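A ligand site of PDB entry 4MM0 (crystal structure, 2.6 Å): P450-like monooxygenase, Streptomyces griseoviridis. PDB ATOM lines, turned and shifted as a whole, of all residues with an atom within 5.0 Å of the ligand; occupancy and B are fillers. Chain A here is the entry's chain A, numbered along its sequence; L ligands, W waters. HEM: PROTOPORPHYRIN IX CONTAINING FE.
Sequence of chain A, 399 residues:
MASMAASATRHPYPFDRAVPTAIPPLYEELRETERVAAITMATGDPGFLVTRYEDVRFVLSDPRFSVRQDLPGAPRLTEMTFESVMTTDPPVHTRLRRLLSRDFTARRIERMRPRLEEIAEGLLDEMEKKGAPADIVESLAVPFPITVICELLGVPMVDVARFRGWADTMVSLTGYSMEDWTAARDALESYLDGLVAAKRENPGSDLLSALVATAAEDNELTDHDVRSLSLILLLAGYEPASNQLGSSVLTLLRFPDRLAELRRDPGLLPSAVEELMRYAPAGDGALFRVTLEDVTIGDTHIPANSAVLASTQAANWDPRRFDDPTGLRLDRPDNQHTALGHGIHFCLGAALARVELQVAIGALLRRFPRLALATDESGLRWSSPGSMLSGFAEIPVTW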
ATOM      1  N   LEU A  60      -4.524  -0.043  -5.828  1.00  0.00           N
ATOM      2  CA  LEU A  60      -3.324   0.669  -5.374  1.00  0.00           C
ATOM      3  C   LEU A  60      -3.586   1.527  -4.136  1.00  0.00           C
ATOM      4  O   LEU A  60      -2.667   1.832  -3.382  1.00  0.00           O
ATOM      5  CB  LEU A  60      -2.748   1.543  -6.489  1.00  0.00           C
ATOM      6  CG  LEU A  60      -2.153   0.837  -7.714  1.00  0.00           C
ATOM      7  CD1 LEU A  60      -1.772   1.856  -8.805  1.00  0.00           C
ATOM      8  CD2 LEU A  60      -0.979  -0.022  -7.309  1.00  0.00           C
ATOM      9  N   VAL A  67       1.279  -3.676   0.729  1.00  0.00           N
ATOM     10  CA  VAL A  67       2.390  -3.607  -0.212  1.00  0.00           C
ATOM     11  C   VAL A  67       3.462  -4.568   0.234  1.00  0.00           C
ATOM     12  O   VAL A  67       4.455  -4.772  -0.486  1.00  0.00           O
ATOM     13  CB  VAL A  67       3.022  -2.191  -0.354  1.00  0.00           C
ATOM     14  CG1 VAL A  67       1.984  -1.177  -0.836  1.00  0.00           C
ATOM     15  CG2 VAL A  67       3.697  -1.739   0.959  1.00  0.00           C
ATOM     16  N   MET A  86      10.590   1.011   3.697  1.00  0.00           N
ATOM     17  CA  MET A  86       9.520   1.883   3.238  1.00  0.00           C
ATOM     18  C   MET A  86       8.397   1.136   2.520  1.00  0.00           C
ATOM     19  O   MET A  86       7.248   1.604   2.505  1.00  0.00           O
ATOM     20  CB  MET A  86      10.031   3.023   2.367  1.00  0.00           C
ATOM     21  CG  MET A  86       8.980   4.125   2.251  1.00  0.00           C
ATOM     22  SD  MET A  86       9.687   5.622   1.626  1.00  0.00           S
ATOM     23  CE  MET A  86       8.435   6.782   2.140  1.00  0.00           C
ATOM     24  N   HIS A  93       4.882   2.893   7.759  1.00  0.00           N
ATOM     25  CA  HIS A  93       5.035   3.579   6.470  1.00  0.00           C
ATOM     26  C   HIS A  93       4.828   5.076   6.647  1.00  0.00           C
ATOM     27  O   HIS A  93       5.670   5.868   6.204  1.00  0.00           O
ATOM     28  CB  HIS A  93       4.092   3.041   5.380  1.00  0.00           C
ATOM     29  CG  HIS A  93       3.983   3.945   4.204  1.00  0.00           C
ATOM     30  ND1 HIS A  93       2.991   4.888   4.076  1.00  0.00           N
ATOM     31  CD2 HIS A  93       4.764   4.071   3.097  1.00  0.00           C
ATOM     32  CE1 HIS A  93       3.152   5.550   2.941  1.00  0.00           C
ATOM     33  NE2 HIS A  93       4.221   5.070   2.328  1.00  0.00           N
ATOM     34  N   ARG A  97       7.397   8.036   5.603  1.00  0.00           N
ATOM     35  CA  ARG A  97       6.883   9.022   4.655  1.00  0.00           C
ATOM     36  C   ARG A  97       7.044  10.419   5.260  1.00  0.00           C
ATOM     37  O   ARG A  97       7.658  11.290   4.647  1.00  0.00           O
ATOM     38  CB  ARG A  97       5.408   8.748   4.361  1.00  0.00           C
ATOM     39  CG  ARG A  97       4.828   9.544   3.210  1.00  0.00           C
ATOM     40  CD  ARG A  97       5.148   8.935   1.863  1.00  0.00           C
ATOM     41  NE  ARG A  97       4.673   9.751   0.756  1.00  0.00           N
ATOM     42  CZ  ARG A  97       4.666   9.379  -0.533  1.00  0.00           C
ATOM     43  NH1 ARG A  97       5.111   8.171  -0.868  1.00  0.00           N
ATOM     44  NH2 ARG A  97       4.212  10.205  -1.469  1.00  0.00           N
ATOM     45  N   PHE A 104      10.639  16.582  -0.739  1.00  0.00           N
ATOM     46  CA  PHE A 104      10.255  16.142  -2.080  1.00  0.00           C
ATOM     47  C   PHE A 104       9.024  16.836  -2.675  1.00  0.00           C
ATOM     48  O   PHE A 104       8.514  16.433  -3.721  1.00  0.00           O
ATOM     49  CB  PHE A 104      10.115  14.612  -2.125  1.00  0.00           C
ATOM     50  CG  PHE A 104      11.441  13.874  -2.062  1.00  0.00           C
ATOM     51  CD1 PHE A 104      12.143  13.580  -3.220  1.00  0.00           C
ATOM     52  CD2 PHE A 104      11.970  13.470  -0.849  1.00  0.00           C
ATOM     53  CE1 PHE A 104      13.356  12.914  -3.168  1.00  0.00           C
ATOM     54  CE2 PHE A 104      13.192  12.793  -0.806  1.00  0.00           C
ATOM     55  CZ  PHE A 104      13.876  12.515  -1.958  1.00  0.00           C
ATOM     56  N   ILE A 149      20.226  11.799  -8.749  1.00  0.00           N
ATOM     57  CA  ILE A 149      19.942  11.062  -7.517  1.00  0.00           C
ATOM     58  C   ILE A 149      21.213  10.847  -6.660  1.00  0.00           C
ATOM     59  O   ILE A 149      21.153  10.980  -5.433  1.00  0.00           O
ATOM     60  CB  ILE A 149      19.137   9.740  -7.773  1.00  0.00           C
ATOM     61  CG1 ILE A 149      18.521   9.223  -6.468  1.00  0.00           C
ATOM     62  CG2 ILE A 149      19.995   8.649  -8.428  1.00  0.00           C
ATOM     63  CD1 ILE A 149      17.522  10.160  -5.871  1.00  0.00           C
ATOM     64  N   ILE A 232      16.431   2.231  -1.323  1.00  0.00           N
ATOM     65  CA  ILE A 232      15.208   2.421  -2.122  1.00  0.00           C
ATOM     66  C   ILE A 232      15.216   3.746  -2.888  1.00  0.00           C
ATOM     67  O   ILE A 232      14.824   3.789  -4.055  1.00  0.00           O
ATOM     68  CB  ILE A 232      13.897   2.214  -1.317  1.00  0.00           C
ATOM     69  CG1 ILE A 232      12.748   1.846  -2.262  1.00  0.00           C
ATOM     70  CG2 ILE A 232      13.524   3.442  -0.502  1.00  0.00           C
ATOM     71  CD1 ILE A 232      13.016   0.569  -3.045  1.00  0.00           C
ATOM     72  N   LEU A 233      15.703   4.815  -2.259  1.00  0.00           N
ATOM     73  CA  LEU A 233      15.801   6.106  -2.934  1.00  0.00           C
ATOM     74  C   LEU A 233      16.735   6.045  -4.138  1.00  0.00           C
ATOM     75  O   LEU A 233      16.480   6.694  -5.152  1.00  0.00           O
ATOM     76  CB  LEU A 233      16.240   7.206  -1.964  1.00  0.00           C
ATOM     77  CG  LEU A 233      15.238   7.537  -0.864  1.00  0.00           C
ATOM     78  CD1 LEU A 233      15.900   8.380   0.209  1.00  0.00           C
ATOM     79  CD2 LEU A 233      14.010   8.259  -1.425  1.00  0.00           C
ATOM     80  N   ALA A 236      14.809   3.445  -6.924  1.00  0.00           N
ATOM     81  CA  ALA A 236      13.638   4.154  -7.431  1.00  0.00           C
ATOM     82  C   ALA A 236      13.997   5.493  -8.070  1.00  0.00           C
ATOM     83  O   ALA A 236      13.336   5.932  -9.002  1.00  0.00           O
ATOM     84  CB  ALA A 236      12.622   4.358  -6.329  1.00  0.00           C
ATOM     85  N   GLY A 237      15.055   6.126  -7.567  1.00  0.00           N
ATOM     86  CA  GLY A 237      15.478   7.424  -8.060  1.00  0.00           C
ATOM     87  C   GLY A 237      16.213   7.338  -9.389  1.00  0.00           C
ATOM     88  O   GLY A 237      16.307   8.336 -10.117  1.00  0.00           O
ATOM     89  N   PRO A 240      13.516   3.799 -12.826  1.00  0.00           N
ATOM     90  CA  PRO A 240      12.347   4.160 -13.627  1.00  0.00           C
ATOM     91  C   PRO A 240      12.580   5.456 -14.412  1.00  0.00           C
ATOM     92  O   PRO A 240      12.164   5.550 -15.566  1.00  0.00           O
ATOM     93  CB  PRO A 240      11.234   4.355 -12.573  1.00  0.00           C
ATOM     94  CG  PRO A 240      11.713   3.602 -11.385  1.00  0.00           C
ATOM     95  CD  PRO A 240      13.202   3.760 -11.380  1.00  0.00           C
ATOM     96  N   ALA A 241      13.246   6.426 -13.790  1.00  0.00           N
ATOM     97  CA  ALA A 241      13.503   7.706 -14.446  1.00  0.00           C
ATOM     98  C   ALA A 241      14.358   7.522 -15.698  1.00  0.00           C
ATOM     99  O   ALA A 241      14.131   8.160 -16.734  1.00  0.00           O
ATOM    100  CB  ALA A 241      14.189   8.673 -13.490  1.00  0.00           C
ATOM    101  N   GLN A 244      12.241   5.917 -18.290  1.00  0.00           N
ATOM    102  CA  GLN A 244      11.235   6.884 -18.707  1.00  0.00           C
ATOM    103  C   GLN A 244      11.802   7.952 -19.638  1.00  0.00           C
ATOM    104  O   GLN A 244      11.138   8.311 -20.620  1.00  0.00           O
ATOM    105  CB  GLN A 244      10.531   7.536 -17.504  1.00  0.00           C
ATOM    106  CG  GLN A 244       9.279   8.326 -17.879  1.00  0.00           C
ATOM    107  CD  GLN A 244       8.214   7.435 -18.498  1.00  0.00           C
ATOM    108  OE1 GLN A 244       7.857   6.398 -17.937  1.00  0.00           O
ATOM    109  NE2 GLN A 244       7.703   7.828 -19.679  1.00  0.00           N
ATOM    110  N   MET A 277       4.347   9.947 -19.839  1.00  0.00           N
ATOM    111  CA  MET A 277       4.291   8.909 -18.812  1.00  0.00           C
ATOM    112  C   MET A 277       3.050   8.039 -18.978  1.00  0.00           C
ATOM    113  O   MET A 277       3.075   6.841 -18.706  1.00  0.00           O
ATOM    114  CB  MET A 277       4.355   9.505 -17.399  1.00  0.00           C
ATOM    115  CG  MET A 277       5.760   9.774 -16.883  1.00  0.00           C
ATOM    116  SD  MET A 277       5.749  10.480 -15.217  1.00  0.00           S
ATOM    117  CE  MET A 277       4.979  12.084 -15.497  1.00  0.00           C
ATOM    118  N   ALA A 282       7.478   2.985 -17.757  1.00  0.00           N
ATOM    119  CA  ALA A 282       8.887   2.851 -17.383  1.00  0.00           C
ATOM    120  C   ALA A 282       9.255   1.382 -17.253  1.00  0.00           C
ATOM    121  O   ALA A 282      10.388   1.052 -16.943  1.00  0.00           O
ATOM    122  CB  ALA A 282       9.179   3.584 -16.081  1.00  0.00           C
ATOM    123  N   LEU A 287       2.063  -3.550 -10.679  1.00  0.00           N
ATOM    124  CA  LEU A 287       2.351  -3.272  -9.275  1.00  0.00           C
ATOM    125  C   LEU A 287       1.721  -4.354  -8.361  1.00  0.00           C
ATOM    126  O   LEU A 287       0.622  -4.854  -8.633  1.00  0.00           O
ATOM    127  CB  LEU A 287       1.863  -1.879  -8.899  1.00  0.00           C
ATOM    128  CG  LEU A 287       2.543  -0.792  -9.721  1.00  0.00           C
ATOM    129  CD1 LEU A 287       2.085   0.609  -9.314  1.00  0.00           C
ATOM    130  CD2 LEU A 287       4.069  -0.923  -9.624  1.00  0.00           C
ATOM    131  N   ARG A 289       0.230  -6.148  -4.906  1.00  0.00           N
ATOM    132  CA  ARG A 289      -0.467  -6.067  -3.616  1.00  0.00           C
ATOM    133  C   ARG A 289      -0.815  -7.462  -3.084  1.00  0.00           C
ATOM    134  O   ARG A 289      -0.870  -8.430  -3.835  1.00  0.00           O
ATOM    135  CB  ARG A 289      -1.738  -5.220  -3.746  1.00  0.00           C
ATOM    136  CG  ARG A 289      -1.501  -3.739  -4.066  1.00  0.00           C
ATOM    137  CD  ARG A 289      -0.691  -3.045  -2.997  1.00  0.00           C
ATOM    138  NE  ARG A 289      -0.570  -1.607  -3.219  1.00  0.00           N
ATOM    139  CZ  ARG A 289       0.430  -1.012  -3.878  1.00  0.00           C
ATOM    140  NH1 ARG A 289       1.412  -1.733  -4.421  1.00  0.00           N
ATOM    141  NH2 ARG A 289       0.438   0.308  -3.998  1.00  0.00           N
ATOM    142  N   THR A 338      -1.753   6.726 -14.031  1.00  0.00           N
ATOM    143  CA  THR A 338      -1.354   5.952 -12.861  1.00  0.00           C
ATOM    144  C   THR A 338       0.143   5.613 -12.843  1.00  0.00           C
ATOM    145  O   THR A 338       0.579   4.840 -11.998  1.00  0.00           O
ATOM    146  CB  THR A 338      -2.142   4.618 -12.787  1.00  0.00           C
ATOM    147  OG1 THR A 338      -1.863   3.837 -13.957  1.00  0.00           O
ATOM    148  CG2 THR A 338      -3.639   4.884 -12.731  1.00  0.00           C
ATOM    149  N   ALA A 339       0.896   6.176 -13.789  1.00  0.00           N
ATOM    150  CA  ALA A 339       2.311   5.821 -13.956  1.00  0.00           C
ATOM    151  C   ALA A 339       3.121   6.138 -12.711  1.00  0.00           C
ATOM    152  O   ALA A 339       4.159   5.528 -12.457  1.00  0.00           O
ATOM    153  CB  ALA A 339       2.903   6.527 -15.171  1.00  0.00           C
ATOM    154  N   LEU A 340       2.650   7.098 -11.926  1.00  0.00           N
ATOM    155  CA  LEU A 340       3.331   7.444 -10.688  1.00  0.00           C
ATOM    156  C   LEU A 340       2.659   6.836  -9.467  1.00  0.00           C
ATOM    157  O   LEU A 340       3.017   7.178  -8.351  1.00  0.00           O
ATOM    158  CB  LEU A 340       3.473   8.976 -10.558  1.00  0.00           C
ATOM    159  CG  LEU A 340       4.498   9.552 -11.543  1.00  0.00           C
ATOM    160  CD1 LEU A 340       4.458  11.071 -11.620  1.00  0.00           C
ATOM    161  CD2 LEU A 340       5.920   9.063 -11.206  1.00  0.00           C
ATOM    162  N   GLY A 341       1.713   5.913  -9.677  1.00  0.00           N
ATOM    163  CA  GLY A 341       0.997   5.297  -8.568  1.00  0.00           C
ATOM    164  C   GLY A 341      -0.228   6.084  -8.089  1.00  0.00           C
ATOM    165  O   GLY A 341      -0.630   7.065  -8.720  1.00  0.00           O
ATOM    166  N   ILE A 344      -1.456   6.286  -0.709  1.00  0.00           N
ATOM    167  CA  ILE A 344      -0.401   6.579   0.266  1.00  0.00           C
ATOM    168  C   ILE A 344       1.011   6.265  -0.250  1.00  0.00           C
ATOM    169  O   ILE A 344       1.987   6.896   0.179  1.00  0.00           O
ATOM    170  CB  ILE A 344      -0.642   5.871   1.617  1.00  0.00           C
ATOM    171  CG1 ILE A 344      -0.446   4.358   1.501  1.00  0.00           C
ATOM    172  CG2 ILE A 344      -2.017   6.205   2.161  1.00  0.00           C
ATOM    173  CD1 ILE A 344      -0.821   3.638   2.768  1.00  0.00           C
ATOM    174  N   HIS A 345       1.137   5.308  -1.155  1.00  0.00           N
ATOM    175  CA  HIS A 345       2.458   5.001  -1.711  1.00  0.00           C
ATOM    176  C   HIS A 345       2.799   5.778  -2.994  1.00  0.00           C
ATOM    177  O   HIS A 345       3.827   5.489  -3.622  1.00  0.00           O
ATOM    178  CB  HIS A 345       2.654   3.500  -1.896  1.00  0.00           C
ATOM    179  CG  HIS A 345       2.772   2.749  -0.609  1.00  0.00           C
ATOM    180  ND1 HIS A 345       1.685   2.206   0.038  1.00  0.00           N
ATOM    181  CD2 HIS A 345       3.844   2.481   0.174  1.00  0.00           C
ATOM    182  CE1 HIS A 345       2.082   1.616   1.153  1.00  0.00           C
ATOM    183  NE2 HIS A 345       3.396   1.771   1.246  1.00  0.00           N
ATOM    184  N   PHE A 346       1.954   6.733  -3.367  1.00  0.00           N
ATOM    185  CA  PHE A 346       2.172   7.585  -4.544  1.00  0.00           C
ATOM    186  C   PHE A 346       3.629   8.059  -4.573  1.00  0.00           C
ATOM    187  O   PHE A 346       4.151   8.528  -3.549  1.00  0.00           O
ATOM    188  CB  PHE A 346       1.222   8.795  -4.508  1.00  0.00           C
ATOM    189  CG  PHE A 346       1.351   9.721  -5.693  1.00  0.00           C
ATOM    190  CD1 PHE A 346       0.784   9.386  -6.920  1.00  0.00           C
ATOM    191  CD2 PHE A 346       2.030  10.923  -5.571  1.00  0.00           C
ATOM    192  CE1 PHE A 346       0.899  10.239  -8.025  1.00  0.00           C
ATOM    193  CE2 PHE A 346       2.153  11.787  -6.681  1.00  0.00           C
ATOM    194  CZ  PHE A 346       1.590  11.439  -7.908  1.00  0.00           C
ATOM    195  N   CYS A 347       4.257   7.912  -5.732  1.00  0.00           N
ATOM    196  CA  CYS A 347       5.689   8.170  -5.923  1.00  0.00           C
ATOM    197  C   CYS A 347       6.229   9.393  -5.169  1.00  0.00           C
ATOM    198  O   CYS A 347       5.807  10.548  -5.412  1.00  0.00           O
ATOM    199  CB  CYS A 347       6.024   8.317  -7.408  1.00  0.00           C
ATOM    200  SG  CYS A 347       7.759   8.845  -7.675  1.00  0.00           S
ATOM    201  N   LEU A 348       7.174   9.114  -4.272  1.00  0.00           N
ATOM    202  CA  LEU A 348       7.856  10.123  -3.485  1.00  0.00           C
ATOM    203  C   LEU A 348       8.568  11.135  -4.371  1.00  0.00           C
ATOM    204  O   LEU A 348       8.716  12.310  -3.995  1.00  0.00           O
ATOM    205  CB  LEU A 348       8.871   9.460  -2.565  1.00  0.00           C
ATOM    206  CG  LEU A 348       9.487  10.314  -1.455  1.00  0.00           C
ATOM    207  CD1 LEU A 348       8.470  10.555  -0.355  1.00  0.00           C
ATOM    208  CD2 LEU A 348      10.707   9.612  -0.905  1.00  0.00           C
ATOM    209  N   GLY A 349       9.015  10.680  -5.536  1.00  0.00           N
ATOM    210  CA  GLY A 349       9.788  11.512  -6.440  1.00  0.00           C
ATOM    211  C   GLY A 349       8.992  12.056  -7.613  1.00  0.00           C
ATOM    212  O   GLY A 349       9.571  12.352  -8.670  1.00  0.00           O
ATOM    213  N   LEU A 352      10.220  15.460  -8.600  1.00  0.00           N
ATOM    214  CA  LEU A 352      11.560  15.219  -9.137  1.00  0.00           C
ATOM    215  C   LEU A 352      11.517  14.601 -10.545  1.00  0.00           C
ATOM    216  O   LEU A 352      12.233  15.056 -11.437  1.00  0.00           O
ATOM    217  CB  LEU A 352      12.382  14.332  -8.193  1.00  0.00           C
ATOM    218  CG  LEU A 352      13.883  14.100  -8.477  1.00  0.00           C
ATOM    219  CD1 LEU A 352      14.582  15.370  -8.934  1.00  0.00           C
ATOM    220  CD2 LEU A 352      14.583  13.553  -7.229  1.00  0.00           C
ATOM    221  N   ALA A 353      10.693  13.569 -10.727  1.00  0.00           N
ATOM    222  CA  ALA A 353      10.607  12.911 -12.028  1.00  0.00           C
ATOM    223  C   ALA A 353      10.100  13.901 -13.078  1.00  0.00           C
ATOM    224  O   ALA A 353      10.639  13.967 -14.191  1.00  0.00           O
ATOM    225  CB  ALA A 353       9.723  11.702 -11.962  1.00  0.00           C
ATOM    226  N   GLU A 356      12.832  16.464 -13.891  1.00  0.00           N
ATOM    227  CA  GLU A 356      13.893  15.796 -14.637  1.00  0.00           C
ATOM    228  C   GLU A 356      13.507  15.660 -16.105  1.00  0.00           C
ATOM    229  O   GLU A 356      14.234  16.119 -16.989  1.00  0.00           O
ATOM    230  CB  GLU A 356      14.212  14.422 -14.015  1.00  0.00           C
ATOM    231  CG  GLU A 356      15.219  14.516 -12.851  1.00  0.00           C
ATOM    232  CD  GLU A 356      15.558  13.173 -12.233  1.00  0.00           C
ATOM    233  OE1 GLU A 356      15.548  12.136 -12.954  1.00  0.00           O
ATOM    234  OE2 GLU A 356      15.846  13.133 -11.019  1.00  0.00           O
HETATM  235  CHA HEM L   1       6.976   4.911  -5.515  1.00  0.00           C
HETATM  236  CHB HEM L   1      11.127   7.477  -5.427  1.00  0.00           C
HETATM  237  CHC HEM L   1      10.776   8.208 -10.227  1.00  0.00           C
HETATM  238  CHD HEM L   1       6.930   5.330 -10.395  1.00  0.00           C
HETATM  239  C1A HEM L   1       8.149   5.478  -5.084  1.00  0.00           C
HETATM  240  C2A HEM L   1       8.736   5.374  -3.760  1.00  0.00           C
HETATM  241  C3A HEM L   1       9.875   6.075  -3.741  1.00  0.00           C
HETATM  242  C4A HEM L   1      10.073   6.657  -5.047  1.00  0.00           C
HETATM  243  CMA HEM L   1      10.823   6.249  -2.529  1.00  0.00           C
HETATM  244  CAA HEM L   1       8.112   4.600  -2.595  1.00  0.00           C
HETATM  245  CBA HEM L   1       7.061   5.542  -2.015  1.00  0.00           C
HETATM  246  CGA HEM L   1       6.305   4.938  -0.855  1.00  0.00           C
HETATM  247  O1A HEM L   1       6.208   3.691  -0.742  1.00  0.00           O
HETATM  248  O2A HEM L   1       5.784   5.724  -0.019  1.00  0.00           O
HETATM  249  C1B HEM L   1      11.345   7.973  -6.698  1.00  0.00           C
HETATM  250  C2B HEM L   1      12.333   8.973  -7.076  1.00  0.00           C
HETATM  251  C3B HEM L   1      12.204   9.156  -8.405  1.00  0.00           C
HETATM  252  C4B HEM L   1      11.163   8.294  -8.893  1.00  0.00           C
HETATM  253  CMB HEM L   1      13.290   9.650  -6.057  1.00  0.00           C
HETATM  254  CAB HEM L   1      12.946  10.075  -9.409  1.00  0.00           C
HETATM  255  CBB HEM L   1      13.943  10.889  -9.093  1.00  0.00           C
HETATM  256  C1C HEM L   1       9.755   7.460 -10.718  1.00  0.00           C
HETATM  257  C2C HEM L   1       9.386   7.302 -12.110  1.00  0.00           C
HETATM  258  C3C HEM L   1       8.305   6.480 -12.143  1.00  0.00           C
HETATM  259  C4C HEM L   1       7.978   6.134 -10.784  1.00  0.00           C
HETATM  260  CMC HEM L   1      10.132   7.979 -13.291  1.00  0.00           C
HETATM  261  CAC HEM L   1       7.481   5.958 -13.349  1.00  0.00           C
HETATM  262  CBC HEM L   1       7.611   6.376 -14.611  1.00  0.00           C
HETATM  263  C1D HEM L   1       6.551   5.001  -9.122  1.00  0.00           C
HETATM  264  C2D HEM L   1       5.355   4.254  -8.804  1.00  0.00           C
HETATM  265  C3D HEM L   1       5.353   4.112  -7.276  1.00  0.00           C
HETATM  266  C4D HEM L   1       6.547   4.792  -6.824  1.00  0.00           C
HETATM  267  CMD HEM L   1       4.317   3.713  -9.819  1.00  0.00           C
HETATM  268  CAD HEM L   1       4.291   3.390  -6.440  1.00  0.00           C
HETATM  269  CBD HEM L   1       4.684   1.950  -6.178  1.00  0.00           C
HETATM  270  CGD HEM L   1       3.479   1.215  -5.670  1.00  0.00           C
HETATM  271  O1D HEM L   1       2.398   1.853  -5.605  1.00  0.00           O
HETATM  272  O2D HEM L   1       3.588   0.013  -5.338  1.00  0.00           O
HETATM  273  NA  HEM L   1       9.001   6.276  -5.842  1.00  0.00           N
HETATM  274  NB  HEM L   1      10.646   7.605  -7.833  1.00  0.00           N
HETATM  275  NC  HEM L   1       8.872   6.747  -9.941  1.00  0.00           N
HETATM  276  ND  HEM L   1       7.224   5.295  -7.940  1.00  0.00           N
HETATM  277 FE   HEM L   1       8.887   6.615  -7.848  1.00  0.00          FE
HETATM  278  O   HOH W   1       5.584  -1.553  -6.024  1.00  0.00           O
HETATM  279  O   HOH W   2       4.971  -0.487  -2.988  1.00  0.00           O
HETATM  280  O   HOH W   3       0.953   4.033  -5.515  1.00  0.00           O
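NH1 of Arg 97 is in salt-bridge range of O2A of the ligand, at 2.7 Å. NE2 of His 93 is in hydrogen-bond range of O2A of the ligand. NH1 of Arg 289 is in salt-bridge range of O2D of the ligand, at 2.9 Å. The side-chain sulfur (SG) of Cys 347 is bound to an iron atom (FE) of the ligand, 2.5 Å away.
The backbone NH (N) of Gly 349 sits close to the side-chain sulfur (SG) of Cys 347 (3.1 Å). The side-chain amide oxygen (OE1) of Gln 244 is in hydrogen-bond range of the backbone NH (N) of Ala 282, 3.4 Å away. NH2 of Arg 97 lies within hydrogen-bond range of O of Phe 346. N of Cys 347 lies within hydrogen-bond range of O of Leu 340, 3.0 Å away.
The backbone carbonyl oxygen (O) of Ala 236 sits close to a nitrogen (NB) of the ligand (3.4 Å). Met 86 touches the ligand (CE to O2A, 3.6 Å). CD2 of Leu 233 touches CMA of the ligand, 3.9 Å away. O of Gly 237 touches CBB of the ligand, 3.6 Å away. CB of Pro 240 touches C2C of the ligand (3.5 Å). Ala 241 touches the ligand. Gln 244 touches the ligand (OE1 to CBC, 3.3 Å). Ala 282 touches the ligand. CD1 of Leu 287 touches CMD of the ligand, at 3.9 Å. Ala 339 touches the ligand. Leu 340 touches the ligand. Gly 341 touches the ligand (N to CMD, 3.4 Å). Ile 344 touches the ligand (O to O2A, 3.98 Å). His 345 touches the ligand (CD2 to O1A, 2.8 Å). CB of Leu 348 touches C3A of the ligand, 3.7 Å away. CA of Gly 349 touches C2B of the ligand, at 3.7 Å. Leu 352 touches the ligand (CG to CBB, 3.3 Å). Ala 353 touches the ligand (CB to CMC, 3.97 Å). OE2 of Glu 356 touches CBB of the ligand, at 3.5 Å. Hydrophobic or aromatic side chains that line the ligand: Met 86, His 93, Leu 233, Ala 236, Pro 240, Ala 282, Leu 287, Leu 340, His 345, Leu 348, Leu 352 and Ala 353. 23 residues have an atom within 4 Å of the ligand: Met 86, His 93, Arg 97, Leu 233, Ala 236, Gly 237, Pro 240, Ala 241, Gln 244, Ala 282, Leu 287, Arg 289, Ala 339, Leu 340, Gly 341, Ile 344, His 345, Cys 347, Leu 348, Gly 349, Leu 352, Ala 353 and Glu 356. The nearest printed residue that does not touch the ligand is Leu 60 (4.2 Å).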
